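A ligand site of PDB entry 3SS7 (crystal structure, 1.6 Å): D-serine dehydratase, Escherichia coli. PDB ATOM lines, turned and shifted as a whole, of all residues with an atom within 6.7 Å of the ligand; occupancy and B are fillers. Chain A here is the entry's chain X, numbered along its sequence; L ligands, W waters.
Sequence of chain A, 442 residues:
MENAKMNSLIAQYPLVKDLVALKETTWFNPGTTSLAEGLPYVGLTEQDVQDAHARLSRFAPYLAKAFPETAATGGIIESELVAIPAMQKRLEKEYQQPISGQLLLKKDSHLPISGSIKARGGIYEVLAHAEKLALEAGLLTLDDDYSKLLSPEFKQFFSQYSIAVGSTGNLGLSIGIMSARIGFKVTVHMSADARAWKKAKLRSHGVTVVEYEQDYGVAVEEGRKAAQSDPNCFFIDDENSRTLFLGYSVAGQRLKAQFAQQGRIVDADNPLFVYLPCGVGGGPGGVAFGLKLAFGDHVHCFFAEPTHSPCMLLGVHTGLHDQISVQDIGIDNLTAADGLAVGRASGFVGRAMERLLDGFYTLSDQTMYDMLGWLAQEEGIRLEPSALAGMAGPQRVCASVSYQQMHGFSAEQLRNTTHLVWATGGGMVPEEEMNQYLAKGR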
ATOM      1  N   SER A 116      21.064  20.679  -5.585  1.00  0.00           N
ATOM      2  CA  SER A 116      19.699  20.256  -5.327  1.00  0.00           C
ATOM      3  C   SER A 116      19.475  18.825  -5.754  1.00  0.00           C
ATOM      4  O   SER A 116      20.350  18.252  -6.425  1.00  0.00           O
ATOM      5  CB  SER A 116      18.700  21.131  -6.100  1.00  0.00           C
ATOM      6  OG  SER A 116      18.666  20.704  -7.439  1.00  0.00           O
ATOM      7  N   ILE A 117      18.313  18.264  -5.396  1.00  0.00           N
ATOM      8  CA  ILE A 117      17.970  16.917  -5.852  1.00  0.00           C
ATOM      9  C   ILE A 117      18.060  16.728  -7.365  1.00  0.00           C
ATOM     10  O   ILE A 117      18.289  15.628  -7.866  1.00  0.00           O
ATOM     11  CB  ILE A 117      16.596  16.488  -5.328  1.00  0.00           C
ATOM     12  CG1 ILE A 117      16.348  15.004  -5.587  1.00  0.00           C
ATOM     13  CG2 ILE A 117      15.462  17.367  -5.884  1.00  0.00           C
ATOM     14  CD1 ILE A 117      15.069  14.513  -4.927  1.00  0.00           C
ATOM     15  N   LYS A 118      17.927  17.843  -8.098  1.00  0.00           N
ATOM     16  CA  LYS A 118      17.997  17.767  -9.576  1.00  0.00           C
ATOM     17  C   LYS A 118      19.408  17.396 -10.086  1.00  0.00           C
ATOM     18  O   LYS A 118      19.578  17.026 -11.254  1.00  0.00           O
ATOM     19  CB  LYS A 118      17.518  19.071 -10.201  1.00  0.00           C
ATOM     20  CG  LYS A 118      16.143  19.540  -9.714  1.00  0.00           C
ATOM     21  CD  LYS A 118      15.104  18.539 -10.085  1.00  0.00           C
ATOM     22  CE  LYS A 118      13.757  19.227 -10.250  1.00  0.00           C
ATOM     23  NZ  LYS A 118      13.423  19.762  -8.943  1.00  0.00           N
ATOM     24  N   GLY A 169      13.599  27.170 -11.894  1.00  0.00           N
ATOM     25  CA  GLY A 169      14.210  26.663 -10.678  1.00  0.00           C
ATOM     26  C   GLY A 169      15.322  25.668 -10.908  1.00  0.00           C
ATOM     27  O   GLY A 169      16.118  25.783 -11.872  1.00  0.00           O
ATOM     28  N   ASN A 170      15.380  24.699  -9.989  1.00  0.00           N
ATOM     29  CA  ASN A 170      16.500  23.769  -9.980  1.00  0.00           C
ATOM     30  C   ASN A 170      16.601  22.849 -11.202  1.00  0.00           C
ATOM     31  O   ASN A 170      17.709  22.395 -11.558  1.00  0.00           O
ATOM     32  CB  ASN A 170      16.501  22.923  -8.705  1.00  0.00           C
ATOM     33  CG  ASN A 170      16.866  23.744  -7.457  1.00  0.00           C
ATOM     34  OD1 ASN A 170      17.889  24.502  -7.457  1.00  0.00           O
ATOM     35  ND2 ASN A 170      16.039  23.650  -6.422  1.00  0.00           N
ATOM     36  N   LEU A 171      15.466  22.569 -11.846  1.00  0.00           N
ATOM     37  CA  LEU A 171      15.544  21.682 -13.024  1.00  0.00           C
ATOM     38  C   LEU A 171      16.362  22.391 -14.117  1.00  0.00           C
ATOM     39  O   LEU A 171      17.274  21.816 -14.708  1.00  0.00           O
ATOM     40  CB  LEU A 171      14.153  21.291 -13.543  1.00  0.00           C
ATOM     41  CG  LEU A 171      14.239  20.316 -14.705  1.00  0.00           C
ATOM     42  CD1 LEU A 171      14.765  18.917 -14.268  1.00  0.00           C
ATOM     43  CD2 LEU A 171      12.833  20.226 -15.298  1.00  0.00           C
ATOM     44  N   ASP A 238       9.653  16.868 -17.638  1.00  0.00           N
ATOM     45  CA  ASP A 238       9.636  16.366 -16.256  1.00  0.00           C
ATOM     46  C   ASP A 238       8.312  15.644 -15.865  1.00  0.00           C
ATOM     47  O   ASP A 238       8.257  14.985 -14.837  1.00  0.00           O
ATOM     48  CB  ASP A 238      10.064  17.423 -15.218  1.00  0.00           C
ATOM     49  CG  ASP A 238       9.065  18.519 -15.010  1.00  0.00           C
ATOM     50  OD1 ASP A 238       8.098  18.662 -15.796  1.00  0.00           O
ATOM     51  OD2 ASP A 238       9.213  19.255 -13.999  1.00  0.00           O
ATOM     52  N   TYR A 248      16.940   9.762 -10.284  1.00  0.00           N
ATOM     53  CA  TYR A 248      16.685   9.978  -8.881  1.00  0.00           C
ATOM     54  C   TYR A 248      16.810   8.677  -8.061  1.00  0.00           C
ATOM     55  O   TYR A 248      17.252   8.658  -6.908  1.00  0.00           O
ATOM     56  CB  TYR A 248      15.272  10.520  -8.735  1.00  0.00           C
ATOM     57  CG  TYR A 248      15.049  11.916  -9.307  1.00  0.00           C
ATOM     58  CD1 TYR A 248      14.046  12.133 -10.271  1.00  0.00           C
ATOM     59  CD2 TYR A 248      15.778  13.013  -8.825  1.00  0.00           C
ATOM     60  CE1 TYR A 248      13.786  13.405 -10.777  1.00  0.00           C
ATOM     61  CE2 TYR A 248      15.534  14.303  -9.332  1.00  0.00           C
ATOM     62  CZ  TYR A 248      14.523  14.466 -10.305  1.00  0.00           C
ATOM     63  OH  TYR A 248      14.259  15.729 -10.770  1.00  0.00           O
ATOM     64  N   LEU A 276       9.559  13.166   1.803  1.00  0.00           N
ATOM     65  CA  LEU A 276      10.107  13.620   0.523  1.00  0.00           C
ATOM     66  C   LEU A 276       9.275  14.777  -0.032  1.00  0.00           C
ATOM     67  O   LEU A 276       8.106  14.580  -0.355  1.00  0.00           O
ATOM     68  CB  LEU A 276       9.984  12.440  -0.455  1.00  0.00           C
ATOM     69  CG  LEU A 276      10.877  11.235  -0.094  1.00  0.00           C
ATOM     70  CD1 LEU A 276      10.246   9.898  -0.561  1.00  0.00           C
ATOM     71  CD2 LEU A 276      12.283  11.423  -0.613  1.00  0.00           C
ATOM     72  N   PRO A 277       9.858  15.969  -0.180  1.00  0.00           N
ATOM     73  CA  PRO A 277       9.154  17.072  -0.865  1.00  0.00           C
ATOM     74  C   PRO A 277       8.731  16.656  -2.285  1.00  0.00           C
ATOM     75  O   PRO A 277       9.513  15.978  -2.983  1.00  0.00           O
ATOM     76  CB  PRO A 277      10.201  18.205  -0.905  1.00  0.00           C
ATOM     77  CG  PRO A 277      11.171  17.902   0.288  1.00  0.00           C
ATOM     78  CD  PRO A 277      11.201  16.348   0.333  1.00  0.00           C
ATOM     79  N   CYS A 278       7.557  17.099  -2.731  1.00  0.00           N
ATOM     80  CA  CYS A 278       6.963  16.607  -3.984  1.00  0.00           C
ATOM     81  C   CYS A 278       6.441  17.758  -4.841  1.00  0.00           C
ATOM     82  O   CYS A 278       5.562  18.477  -4.409  1.00  0.00           O
ATOM     83  CB  CYS A 278       5.859  15.603  -3.700  1.00  0.00           C
ATOM     84  SG  CYS A 278       5.033  15.007  -5.187  1.00  0.00           S
ATOM     85  N   GLY A 279       7.036  17.900  -6.031  1.00  0.00           N
ATOM     86  CA  GLY A 279       6.575  18.851  -7.059  1.00  0.00           C
ATOM     87  C   GLY A 279       5.680  18.089  -8.014  1.00  0.00           C
ATOM     88  O   GLY A 279       4.563  17.784  -7.677  1.00  0.00           O
ATOM     89  N   VAL A 280       6.210  17.760  -9.163  1.00  0.00           N
ATOM     90  CA  VAL A 280       5.502  16.943 -10.166  1.00  0.00           C
ATOM     91  C   VAL A 280       5.457  15.461  -9.771  1.00  0.00           C
ATOM     92  O   VAL A 280       4.561  14.721 -10.162  1.00  0.00           O
ATOM     93  CB  VAL A 280       6.113  17.147 -11.576  1.00  0.00           C
ATOM     94  CG1 VAL A 280       7.412  16.389 -11.735  1.00  0.00           C
ATOM     95  CG2 VAL A 280       5.153  16.679 -12.679  1.00  0.00           C
ATOM     96  N   GLY A 281       6.484  15.032  -9.032  1.00  0.00           N
ATOM     97  CA  GLY A 281       6.511  13.719  -8.452  1.00  0.00           C
ATOM     98  C   GLY A 281       7.703  12.874  -8.885  1.00  0.00           C
ATOM     99  O   GLY A 281       7.982  11.840  -8.291  1.00  0.00           O
ATOM    100  N   GLY A 282       8.435  13.310  -9.921  1.00  0.00           N
ATOM    101  CA  GLY A 282       9.573  12.533 -10.405  1.00  0.00           C
ATOM    102  C   GLY A 282      10.668  12.309  -9.353  1.00  0.00           C
ATOM    103  O   GLY A 282      11.179  11.180  -9.186  1.00  0.00           O
ATOM    104  N   GLY A 283      11.058  13.405  -8.701  1.00  0.00           N
ATOM    105  CA  GLY A 283      12.133  13.350  -7.686  1.00  0.00           C
ATOM    106  C   GLY A 283      11.770  12.413  -6.530  1.00  0.00           C
ATOM    107  O   GLY A 283      12.454  11.414  -6.251  1.00  0.00           O
ATOM    108  N   PRO A 284      10.704  12.738  -5.785  1.00  0.00           N
ATOM    109  CA  PRO A 284      10.363  11.917  -4.651  1.00  0.00           C
ATOM    110  C   PRO A 284       9.946  10.479  -5.067  1.00  0.00           C
ATOM    111  O   PRO A 284      10.243   9.505  -4.378  1.00  0.00           O
ATOM    112  CB  PRO A 284       9.190  12.712  -4.003  1.00  0.00           C
ATOM    113  CG  PRO A 284       8.571  13.441  -5.188  1.00  0.00           C
ATOM    114  CD  PRO A 284       9.799  13.898  -5.938  1.00  0.00           C
ATOM    115  N   GLY A 285       9.285  10.376  -6.209  1.00  0.00           N
ATOM    116  CA  GLY A 285       8.843   9.054  -6.717  1.00  0.00           C
ATOM    117  C   GLY A 285      10.057   8.177  -7.052  1.00  0.00           C
ATOM    118  O   GLY A 285      10.104   6.973  -6.688  1.00  0.00           O
ATOM    119  N   ASP A 338       8.872  27.325  -4.234  1.00  0.00           N
ATOM    120  CA  ASP A 338       8.818  27.454  -5.690  1.00  0.00           C
ATOM    121  C   ASP A 338       9.132  26.154  -6.398  1.00  0.00           C
ATOM    122  O   ASP A 338       8.530  25.850  -7.418  1.00  0.00           O
ATOM    123  CB  ASP A 338       9.698  28.590  -6.171  1.00  0.00           C
ATOM    124  CG  ASP A 338      11.133  28.428  -5.721  1.00  0.00           C
ATOM    125  OD1 ASP A 338      11.991  28.100  -6.535  1.00  0.00           O
ATOM    126  OD2 ASP A 338      11.378  28.622  -4.504  1.00  0.00           O
ATOM    127  N   GLY A 339      10.009  25.325  -5.818  1.00  0.00           N
ATOM    128  CA  GLY A 339      10.294  24.005  -6.432  1.00  0.00           C
ATOM    129  C   GLY A 339       9.119  23.041  -6.391  1.00  0.00           C
ATOM    130  O   GLY A 339       9.127  21.977  -7.078  1.00  0.00           O
ATOM    131  N   LEU A 340       8.112  23.371  -5.574  1.00  0.00           N
ATOM    132  CA  LEU A 340       6.945  22.506  -5.391  1.00  0.00           C
ATOM    133  C   LEU A 340       5.671  23.154  -5.957  1.00  0.00           C
ATOM    134  O   LEU A 340       4.567  22.616  -5.763  1.00  0.00           O
ATOM    135  CB  LEU A 340       6.712  22.159  -3.899  1.00  0.00           C
ATOM    136  CG  LEU A 340       7.945  21.746  -3.071  1.00  0.00           C
ATOM    137  CD1 LEU A 340       7.511  21.401  -1.621  1.00  0.00           C
ATOM    138  CD2 LEU A 340       8.696  20.605  -3.724  1.00  0.00           C
ATOM    139  N   VAL A 342       3.729  23.107  -8.379  1.00  0.00           N
ATOM    140  CA  VAL A 342       3.308  22.333  -9.561  1.00  0.00           C
ATOM    141  C   VAL A 342       1.820  22.017  -9.388  1.00  0.00           C
ATOM    142  O   VAL A 342       1.411  21.442  -8.384  1.00  0.00           O
ATOM    143  CB  VAL A 342       4.181  21.047  -9.671  1.00  0.00           C
ATOM    144  CG1 VAL A 342       3.757  20.156 -10.843  1.00  0.00           C
ATOM    145  CG2 VAL A 342       5.673  21.464  -9.724  1.00  0.00           C
ATOM    146  N   GLU A 384      16.410  25.985   1.216  1.00  0.00           N
ATOM    147  CA  GLU A 384      15.316  26.750   0.613  1.00  0.00           C
ATOM    148  C   GLU A 384      13.977  26.224   1.147  1.00  0.00           C
ATOM    149  O   GLU A 384      13.892  25.111   1.604  1.00  0.00           O
ATOM    150  CB  GLU A 384      15.381  26.693  -0.913  1.00  0.00           C
ATOM    151  CG  GLU A 384      15.132  25.354  -1.493  1.00  0.00           C
ATOM    152  CD  GLU A 384      15.193  25.382  -3.013  1.00  0.00           C
ATOM    153  OE1 GLU A 384      14.180  25.815  -3.645  1.00  0.00           O
ATOM    154  OE2 GLU A 384      16.225  25.018  -3.606  1.00  0.00           O
ATOM    155  N   SER A 386      11.194  25.041  -0.056  1.00  0.00           N
ATOM    156  CA  SER A 386      10.729  23.743  -0.608  1.00  0.00           C
ATOM    157  C   SER A 386      11.367  22.565   0.126  1.00  0.00           C
ATOM    158  O   SER A 386      10.727  21.490   0.288  1.00  0.00           O
ATOM    159  CB  SER A 386      11.088  23.648  -2.103  1.00  0.00           C
ATOM    160  OG  SER A 386      10.391  24.649  -2.850  1.00  0.00           O
ATOM    161  N   ALA A 387      12.644  22.738   0.490  1.00  0.00           N
ATOM    162  CA  ALA A 387      13.428  21.653   1.067  1.00  0.00           C
ATOM    163  C   ALA A 387      13.023  21.377   2.547  1.00  0.00           C
ATOM    164  O   ALA A 387      13.569  20.457   3.170  1.00  0.00           O
ATOM    165  CB  ALA A 387      14.907  22.019   0.983  1.00  0.00           C
ATOM    166  N   ALA A 423      16.224  16.654   2.308  1.00  0.00           N
ATOM    167  CA  ALA A 423      16.387  18.063   1.925  1.00  0.00           C
ATOM    168  C   ALA A 423      16.768  18.110   0.470  1.00  0.00           C
ATOM    169  O   ALA A 423      17.728  17.440   0.043  1.00  0.00           O
ATOM    170  CB  ALA A 423      17.508  18.710   2.759  1.00  0.00           C
ATOM    171  N   THR A 424      16.050  18.943  -0.275  1.00  0.00           N
ATOM    172  CA  THR A 424      16.121  18.899  -1.745  1.00  0.00           C
ATOM    173  C   THR A 424      16.786  20.108  -2.436  1.00  0.00           C
ATOM    174  O   THR A 424      17.034  20.077  -3.643  1.00  0.00           O
ATOM    175  CB  THR A 424      14.710  18.743  -2.308  1.00  0.00           C
ATOM    176  OG1 THR A 424      13.867  19.718  -1.685  1.00  0.00           O
ATOM    177  CG2 THR A 424      14.171  17.323  -2.065  1.00  0.00           C
ATOM    178  N   GLY A 425      17.103  21.169  -1.674  1.00  0.00           N
ATOM    179  CA  GLY A 425      17.768  22.355  -2.285  1.00  0.00           C
ATOM    180  C   GLY A 425      18.211  23.340  -1.220  1.00  0.00           C
ATOM    181  O   GLY A 425      17.708  23.300  -0.099  1.00  0.00           O
ATOM    182  N   GLY A 426      19.170  24.204  -1.577  1.00  0.00           N
ATOM    183  CA  GLY A 426      19.583  25.288  -0.697  1.00  0.00           C
ATOM    184  C   GLY A 426      21.056  25.633  -0.782  1.00  0.00           C
ATOM    185  O   GLY A 426      21.461  26.794  -0.559  1.00  0.00           O
HETATM  186  N1  LIG L   1      12.490  20.228  -3.893  1.00  0.00           N
HETATM  187  C1  LIG L   1      13.231  21.059  -4.676  1.00  0.00           C
HETATM  188  C2  LIG L   1      14.001  22.191  -4.055  1.00  0.00           C
HETATM  189  C3  LIG L   1      13.248  20.815  -6.045  1.00  0.00           C
HETATM  190  O1  LIG L   1      14.011  21.658  -6.843  1.00  0.00           O
HETATM  191  C4  LIG L   1      12.516  19.710  -6.532  1.00  0.00           C
HETATM  192  C5  LIG L   1      12.694  19.298  -7.948  1.00  0.00           C
HETATM  193  C6  LIG L   1      11.772  18.892  -5.683  1.00  0.00           C
HETATM  194  C7  LIG L   1      11.770  19.174  -4.349  1.00  0.00           C
HETATM  195  C8  LIG L   1      10.952  17.696  -6.143  1.00  0.00           C
HETATM  196  O2  LIG L   1      10.434  17.996  -7.416  1.00  0.00           O
HETATM  197  P1  LIG L   1       9.639  17.000  -8.410  1.00  0.00           P
HETATM  198  O3  LIG L   1       9.023  18.036  -9.337  1.00  0.00           O
HETATM  199  O4  LIG L   1       8.594  16.266  -7.645  1.00  0.00           O
HETATM  200  O5  LIG L   1      10.587  16.073  -9.065  1.00  0.00           O
HETATM  201  O   HOH W   1      13.341  24.213  -8.176  1.00  0.00           O
HETATM  202  O   HOH W   2      11.703  16.103 -11.470  1.00  0.00           O
HETATM  203  O   HOH W   3      10.594  18.649 -11.780  1.00  0.00           O
HETATM  204  O   HOH W   4       9.114  20.679  -9.432  1.00  0.00           O
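Water W4 bridges an oxygen (O3) of the ligand (2.6 Å) and the backbone carbonyl oxygen (O) of Gly 339 (2.7 Å).
Water W2 bridges an oxygen (O5) of the ligand (2.7 Å) and the side-chain hydroxyl of Tyr 248 (2.7 Å).
Water W1 bridges N of Asn 170 and O1 of the ligand.
Water W3 bridges OD2 of Asp 238 and O3 of the ligand.
N of Lys 118 lies close to OG of Ser 116 (3.0 Å).
The backbone carbonyl oxygen (O) of Thr 424 is in hydrogen-bond range of the backbone NH (N) of Ile 117 (2.8 Å).
The side-chain amide nitrogen (ND2) of Asn 170 lies within hydrogen-bond range of the side-chain carboxylate (OE2) of Glu 384 (3.1 Å).
N of Glu 384 lies within hydrogen-bond range of O of Gly 425 (3.3 Å).
The backbone NH (N) of Gly 339 is in hydrogen-bond range of the side-chain hydroxyl (OG) of Ser 386 (3.1 Å).
The backbone NH of Asp 338 sits at hydrogen-bond distance from the side-chain hydroxyl of Ser 386.
NZ of Lys 118 is bonded to C5 of the ligand, 1.3 Å away.
The side-chain hydroxyl of Thr 424 is in hydrogen-bond range of a nitrogen (N1) of the ligand.
The backbone NH of Gly 283 is in hydrogen-bond range of an oxygen (O5) of the ligand, 2.7 Å away.
The backbone NH (N) of Gly 279 sits at hydrogen-bond distance from an oxygen (O4) of the ligand, at 2.8 Å.
An oxygen (O4) of the ligand lies within hydrogen-bond range of the backbone NH (N) of Gly 281.
An oxygen (O3) of the ligand lies within hydrogen-bond range of the backbone NH (N) of Val 280 (2.8 Å).
An oxygen (O1) of the ligand sits at hydrogen-bond distance from the side-chain amide nitrogen (ND2) of Asn 170 (2.9 Å).
Merely in contact with the ligand: Pro 284 (3.2 Å), Leu 340 (3.4 Å), Glu 384 (3.6 Å), Gly 282 (3.6 Å), Ser 386 (3.8 Å), Ile 117 (3.8 Å), Cys 278 (3.8 Å) and Pro 277 (3.9 Å).
Hydrophobic or aromatic side chains within 4 Å of the ligand: Ile 117, Pro 277, Val 280, Pro 284 and Leu 340.
Within 4 Å of the ligand: Ile 117, Lys 118, Asn 170, Pro 277, Cys 278, Gly 279, Val 280, Gly 281, Gly 282, Gly 283, Pro 284, Leu 340, Glu 384, Ser 386 and Thr 424.
The nearest printed residue that does not touch the ligand is Gly 425 (4.04 Å).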
